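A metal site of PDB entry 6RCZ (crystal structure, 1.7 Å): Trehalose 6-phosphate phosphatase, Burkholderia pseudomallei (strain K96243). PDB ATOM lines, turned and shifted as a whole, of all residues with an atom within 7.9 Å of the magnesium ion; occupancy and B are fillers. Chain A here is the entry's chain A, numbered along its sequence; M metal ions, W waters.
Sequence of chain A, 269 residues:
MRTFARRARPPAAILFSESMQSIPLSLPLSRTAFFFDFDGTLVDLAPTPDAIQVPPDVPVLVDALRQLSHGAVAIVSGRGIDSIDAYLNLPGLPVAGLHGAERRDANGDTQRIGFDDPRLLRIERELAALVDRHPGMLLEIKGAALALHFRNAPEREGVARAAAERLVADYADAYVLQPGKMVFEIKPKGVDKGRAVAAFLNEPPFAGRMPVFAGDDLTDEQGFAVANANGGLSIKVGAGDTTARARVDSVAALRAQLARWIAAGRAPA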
ATOM      1  N   ASP A  37      25.523  -1.813   9.364  1.00  0.00           N
ATOM      2  CA  ASP A  37      26.703  -1.005   9.584  1.00  0.00           C
ATOM      3  C   ASP A  37      27.602  -1.088   8.346  1.00  0.00           C
ATOM      4  O   ASP A  37      27.469  -1.982   7.496  1.00  0.00           O
ATOM      5  CB  ASP A  37      27.449  -1.480  10.835  1.00  0.00           C
ATOM      6  CG  ASP A  37      28.746  -0.719  11.093  1.00  0.00           C
ATOM      7  OD1 ASP A  37      28.715   0.537  11.174  1.00  0.00           O
ATOM      8  OD2 ASP A  37      29.793  -1.375  11.244  1.00  0.00           O
ATOM      9  N   PHE A  38      28.530  -0.127   8.217  1.00  0.00           N
ATOM     10  CA  PHE A  38      29.392  -0.070   7.041  1.00  0.00           C
ATOM     11  C   PHE A  38      30.786  -0.615   7.326  1.00  0.00           C
ATOM     12  O   PHE A  38      31.078  -1.771   6.989  1.00  0.00           O
ATOM     13  CB  PHE A  38      29.460   1.370   6.504  1.00  0.00           C
ATOM     14  CG  PHE A  38      29.923   1.441   5.069  1.00  0.00           C
ATOM     15  CD1 PHE A  38      29.193   0.837   4.060  1.00  0.00           C
ATOM     16  CD2 PHE A  38      31.088   2.119   4.741  1.00  0.00           C
ATOM     17  CE1 PHE A  38      29.622   0.908   2.735  1.00  0.00           C
ATOM     18  CE2 PHE A  38      31.518   2.190   3.416  1.00  0.00           C
ATOM     19  CZ  PHE A  38      30.774   1.580   2.408  1.00  0.00           C
ATOM     20  N   ASP A  39      31.662   0.192   7.933  1.00  0.00           N
ATOM     21  CA  ASP A  39      33.035  -0.238   8.198  1.00  0.00           C
ATOM     22  C   ASP A  39      33.085  -1.452   9.115  1.00  0.00           C
ATOM     23  O   ASP A  39      32.457  -1.473  10.172  1.00  0.00           O
ATOM     24  CB  ASP A  39      33.836   0.897   8.824  1.00  0.00           C
ATOM     25  CG  ASP A  39      34.153   1.994   7.838  1.00  0.00           C
ATOM     26  OD1 ASP A  39      35.314   2.133   7.431  1.00  0.00           O
ATOM     27  OD2 ASP A  39      33.209   2.727   7.453  1.00  0.00           O
ATOM     28  N   GLY A  40      33.858  -2.466   8.710  1.00  0.00           N
ATOM     29  CA  GLY A  40      33.978  -3.686   9.478  1.00  0.00           C
ATOM     30  C   GLY A  40      32.810  -4.648   9.332  1.00  0.00           C
ATOM     31  O   GLY A  40      32.858  -5.752   9.887  1.00  0.00           O
ATOM     32  N   THR A  41      31.768  -4.249   8.595  1.00  0.00           N
ATOM     33  CA  THR A  41      30.561  -5.054   8.417  1.00  0.00           C
ATOM     34  C   THR A  41      30.321  -5.374   6.941  1.00  0.00           C
ATOM     35  O   THR A  41      30.306  -6.546   6.561  1.00  0.00           O
ATOM     36  CB  THR A  41      29.370  -4.325   9.033  1.00  0.00           C
ATOM     37  OG1 THR A  41      29.528  -4.297  10.464  1.00  0.00           O
ATOM     38  CG2 THR A  41      28.055  -5.022   8.720  1.00  0.00           C
ATOM     39  N   LEU A  42      30.102  -4.359   6.106  1.00  0.00           N
ATOM     40  CA  LEU A  42      30.009  -4.562   4.661  1.00  0.00           C
ATOM     41  C   LEU A  42      31.345  -4.382   3.963  1.00  0.00           C
ATOM     42  O   LEU A  42      31.504  -4.825   2.818  1.00  0.00           O
ATOM     43  CB  LEU A  42      29.007  -3.568   4.055  1.00  0.00           C
ATOM     44  CG  LEU A  42      27.561  -3.701   4.509  1.00  0.00           C
ATOM     45  CD1 LEU A  42      26.717  -2.597   3.876  1.00  0.00           C
ATOM     46  CD2 LEU A  42      27.036  -5.070   4.132  1.00  0.00           C
ATOM     47  N   VAL A  43      32.281  -3.734   4.632  1.00  0.00           N
ATOM     48  CA  VAL A  43      33.582  -3.420   4.065  1.00  0.00           C
ATOM     49  C   VAL A  43      34.619  -3.642   5.154  1.00  0.00           C
ATOM     50  O   VAL A  43      34.353  -3.444   6.341  1.00  0.00           O
ATOM     51  CB  VAL A  43      33.583  -1.980   3.499  1.00  0.00           C
ATOM     52  CG1 VAL A  43      33.765  -0.950   4.603  1.00  0.00           C
ATOM     53  CG2 VAL A  43      34.616  -1.840   2.439  1.00  0.00           C
ATOM     54  N   LEU A  45      37.685  -3.209   7.702  1.00  0.00           N
ATOM     55  CA  LEU A  45      38.264  -2.092   8.423  1.00  0.00           C
ATOM     56  C   LEU A  45      39.686  -1.840   7.933  1.00  0.00           C
ATOM     57  O   LEU A  45      40.466  -2.767   7.720  1.00  0.00           O
ATOM     58  CB  LEU A  45      38.290  -2.369   9.924  1.00  0.00           C
ATOM     59  CG  LEU A  45      37.194  -1.743  10.788  1.00  0.00           C
ATOM     60  CD1 LEU A  45      37.255  -2.348  12.182  1.00  0.00           C
ATOM     61  CD2 LEU A  45      37.352  -0.242  10.872  1.00  0.00           C
ATOM     62  N   VAL A  76      23.220   1.990   8.738  1.00  0.00           N
ATOM     63  CA  VAL A  76      23.236   2.581  10.077  1.00  0.00           C
ATOM     64  C   VAL A  76      24.699   2.581  10.500  1.00  0.00           C
ATOM     65  O   VAL A  76      25.209   1.602  11.048  1.00  0.00           O
ATOM     66  CB  VAL A  76      22.350   1.805  11.068  1.00  0.00           C
ATOM     67  CG1 VAL A  76      22.201   2.562  12.393  1.00  0.00           C
ATOM     68  CG2 VAL A  76      20.979   1.577  10.458  1.00  0.00           C
ATOM     69  N   SER A  77      25.397   3.687  10.256  1.00  0.00           N
ATOM     70  CA  SER A  77      26.850   3.744  10.332  1.00  0.00           C
ATOM     71  C   SER A  77      27.316   4.789  11.345  1.00  0.00           C
ATOM     72  O   SER A  77      26.551   5.622  11.818  1.00  0.00           O
ATOM     73  CB  SER A  77      27.443   4.053   8.958  1.00  0.00           C
ATOM     74  OG  SER A  77      26.836   5.214   8.451  1.00  0.00           O
ATOM     75  N   GLY A  78      28.617   4.735  11.645  1.00  0.00           N
ATOM     76  CA  GLY A  78      29.268   5.761  12.441  1.00  0.00           C
ATOM     77  C   GLY A  78      29.828   6.830  11.519  1.00  0.00           C
ATOM     78  O   GLY A  78      30.212   7.916  11.973  1.00  0.00           O
ATOM     79  N   HIS A  99      26.299   7.469  14.082  1.00  0.00           N
ATOM     80  CA  HIS A  99      25.685   6.698  15.169  1.00  0.00           C
ATOM     81  C   HIS A  99      24.250   7.132  15.459  1.00  0.00           C
ATOM     82  O   HIS A  99      23.757   6.934  16.571  1.00  0.00           O
ATOM     83  CB  HIS A  99      26.534   6.770  16.449  1.00  0.00           C
ATOM     84  CG  HIS A  99      27.961   6.396  16.240  1.00  0.00           C
ATOM     85  ND1 HIS A  99      28.429   5.102  16.392  1.00  0.00           N
ATOM     86  CD2 HIS A  99      29.040   7.141  15.889  1.00  0.00           C
ATOM     87  CE1 HIS A  99      29.720   5.070  16.139  1.00  0.00           C
ATOM     88  NE2 HIS A  99      30.119   6.300  15.832  1.00  0.00           N
ATOM     89  N   LYS A 181      36.641  -0.063  18.070  1.00  0.00           N
ATOM     90  CA  LYS A 181      37.934  -0.682  17.805  1.00  0.00           C
ATOM     91  C   LYS A 181      39.003   0.389  17.556  1.00  0.00           C
ATOM     92  O   LYS A 181      38.963   1.081  16.538  1.00  0.00           O
ATOM     93  CB  LYS A 181      37.823  -1.643  16.623  1.00  0.00           C
ATOM     94  CG  LYS A 181      36.883  -2.826  16.901  1.00  0.00           C
ATOM     95  CD  LYS A 181      36.460  -3.549  15.640  1.00  0.00           C
ATOM     96  CE  LYS A 181      35.558  -4.718  15.967  1.00  0.00           C
ATOM     97  NZ  LYS A 181      35.407  -5.590  14.770  1.00  0.00           N
ATOM     98  N   LYS A 193      22.373   3.922  17.573  1.00  0.00           N
ATOM     99  CA  LYS A 193      22.000   3.097  16.431  1.00  0.00           C
ATOM    100  C   LYS A 193      20.690   2.376  16.684  1.00  0.00           C
ATOM    101  O   LYS A 193      19.914   2.167  15.739  1.00  0.00           O
ATOM    102  CB  LYS A 193      23.121   2.101  16.104  1.00  0.00           C
ATOM    103  CG  LYS A 193      24.367   2.736  15.502  1.00  0.00           C
ATOM    104  CD  LYS A 193      25.223   1.694  14.774  1.00  0.00           C
ATOM    105  CE  LYS A 193      26.264   2.378  13.918  1.00  0.00           C
ATOM    106  NZ  LYS A 193      27.147   1.410  13.163  1.00  0.00           N
ATOM    107  N   ALA A 214      23.063  -6.142  11.056  1.00  0.00           N
ATOM    108  CA  ALA A 214      24.406  -6.701  11.054  1.00  0.00           C
ATOM    109  C   ALA A 214      25.405  -5.616  11.466  1.00  0.00           C
ATOM    110  O   ALA A 214      25.338  -4.484  10.975  1.00  0.00           O
ATOM    111  CB  ALA A 214      24.760  -7.267   9.662  1.00  0.00           C
ATOM    112  N   GLY A 215      26.322  -5.967  12.371  1.00  0.00           N
ATOM    113  CA  GLY A 215      27.322  -5.016  12.839  1.00  0.00           C
ATOM    114  C   GLY A 215      28.530  -5.721  13.405  1.00  0.00           C
ATOM    115  O   GLY A 215      28.537  -6.941  13.588  1.00  0.00           O
ATOM    116  N   ASP A 216      29.575  -4.941  13.694  1.00  0.00           N
ATOM    117  CA  ASP A 216      30.836  -5.512  14.151  1.00  0.00           C
ATOM    118  C   ASP A 216      31.413  -4.910  15.426  1.00  0.00           C
ATOM    119  O   ASP A 216      32.365  -5.476  15.965  1.00  0.00           O
ATOM    120  CB  ASP A 216      31.899  -5.382  13.040  1.00  0.00           C
ATOM    121  CG  ASP A 216      32.406  -3.960  12.903  1.00  0.00           C
ATOM    122  OD1 ASP A 216      31.585  -3.078  12.597  1.00  0.00           O
ATOM    123  OD2 ASP A 216      33.622  -3.730  13.112  1.00  0.00           O
ATOM    124  N   ASP A 217      30.883  -3.789  15.918  1.00  0.00           N
ATOM    125  CA  ASP A 217      31.552  -3.062  16.984  1.00  0.00           C
ATOM    126  C   ASP A 217      30.549  -2.768  18.107  1.00  0.00           C
ATOM    127  O   ASP A 217      29.369  -3.153  18.044  1.00  0.00           O
ATOM    128  CB  ASP A 217      32.187  -1.772  16.461  1.00  0.00           C
ATOM    129  CG  ASP A 217      33.442  -1.374  17.234  1.00  0.00           C
ATOM    130  OD1 ASP A 217      33.579  -1.778  18.421  1.00  0.00           O
ATOM    131  OD2 ASP A 217      34.286  -0.640  16.670  1.00  0.00           O
ATOM    132  N   LEU A 218      31.042  -2.088  19.145  1.00  0.00           N
ATOM    133  CA  LEU A 218      30.232  -1.880  20.342  1.00  0.00           C
ATOM    134  C   LEU A 218      29.001  -1.031  20.047  1.00  0.00           C
ATOM    135  O   LEU A 218      27.921  -1.288  20.593  1.00  0.00           O
ATOM    136  CB  LEU A 218      31.079  -1.237  21.438  1.00  0.00           C
ATOM    137  CG  LEU A 218      30.306  -0.796  22.678  1.00  0.00           C
ATOM    138  CD1 LEU A 218      29.611  -2.000  23.340  1.00  0.00           C
ATOM    139  CD2 LEU A 218      31.217  -0.046  23.651  1.00  0.00           C
ATOM    140  N   THR A 219      29.137  -0.042  19.171  1.00  0.00           N
ATOM    141  CA  THR A 219      28.001   0.805  18.807  1.00  0.00           C
ATOM    142  C   THR A 219      26.853  -0.010  18.236  1.00  0.00           C
ATOM    143  O   THR A 219      25.690   0.336  18.410  1.00  0.00           O
ATOM    144  CB  THR A 219      28.467   1.878  17.821  1.00  0.00           C
ATOM    145  OG1 THR A 219      27.378   2.748  17.489  1.00  0.00           O
ATOM    146  CG2 THR A 219      29.028   1.252  16.537  1.00  0.00           C
ATOM    147  N   ASP A 220      27.173  -1.134  17.582  1.00  0.00           N
ATOM    148  CA  ASP A 220      26.158  -1.955  16.928  1.00  0.00           C
ATOM    149  C   ASP A 220      25.352  -2.798  17.900  1.00  0.00           C
ATOM    150  O   ASP A 220      24.284  -3.311  17.522  1.00  0.00           O
ATOM    151  CB  ASP A 220      26.835  -2.828  15.869  1.00  0.00           C
ATOM    152  CG  ASP A 220      27.627  -1.999  14.866  1.00  0.00           C
ATOM    153  OD1 ASP A 220      27.034  -1.127  14.216  1.00  0.00           O
ATOM    154  OD2 ASP A 220      28.854  -2.206  14.751  1.00  0.00           O
ATOM    155  N   VAL A 237      29.458  -9.559  13.160  1.00  0.00           N
ATOM    156  CA  VAL A 237      30.534  -9.853  12.209  1.00  0.00           C
ATOM    157  C   VAL A 237      31.844  -9.892  12.980  1.00  0.00           C
ATOM    158  O   VAL A 237      32.225  -8.895  13.608  1.00  0.00           O
ATOM    159  CB  VAL A 237      30.584  -8.800  11.093  1.00  0.00           C
ATOM    160  CG1 VAL A 237      31.691  -9.121  10.105  1.00  0.00           C
ATOM    161  CG2 VAL A 237      29.242  -8.708  10.376  1.00  0.00           C
HETATM  162 MG    MG M   1      31.661  -1.091  12.078  1.00  0.00          MG
HETATM  163  O   HOH W   1      33.663  -1.070  12.841  1.00  0.00           O
HETATM  164  O   HOH W   2      30.813  -0.513  13.790  1.00  0.00           O
HETATM  165  O   HOH W   3      31.846   0.929  11.767  1.00  0.00           O
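N of Asp 37 sits at hydrogen-bond distance from O of Ala 214, 3.1 Å away. N of Asp 216 lies within hydrogen-bond range of OG1 of Thr 41 (3.3 Å). NZ of Lys 181 lies within salt-bridge range of OD2 of Asp 216 (3.1 Å). The side-chain amino group (NZ) of Lys 193 is in salt-bridge range of the side-chain carboxylate (OD1) of Asp 37, 2.7 Å away. The side-chain carboxylate (OD2) of Asp 37 sits close to the side-chain hydroxyl (OG1) of Thr 41 (3.0 Å). The backbone NH (N) of Asp 216 lies within hydrogen-bond range of the side-chain carboxylate (OD2) of Asp 220, at 3.0 Å.
Three residues have an atom within 4 Å of the magnesium ion: Asp 37, Asp 39 and Asp 216. The nearest printed residue that does not touch the magnesium ion is Asp 220 (4.03 Å).
The magnesium ion is bound by water W2 (2.0 Å), water W3 (2.1 Å), the side-chain carboxylate (OD1) of Asp 216 (2.1 Å), the side-chain carboxylate (OD2) of Asp 37 (2.1 Å), the backbone carbonyl oxygen (O) of Asp 39 (2.1 Å) and water W1 (2.1 Å). The magnesium ion has six donor atoms within binding distance.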
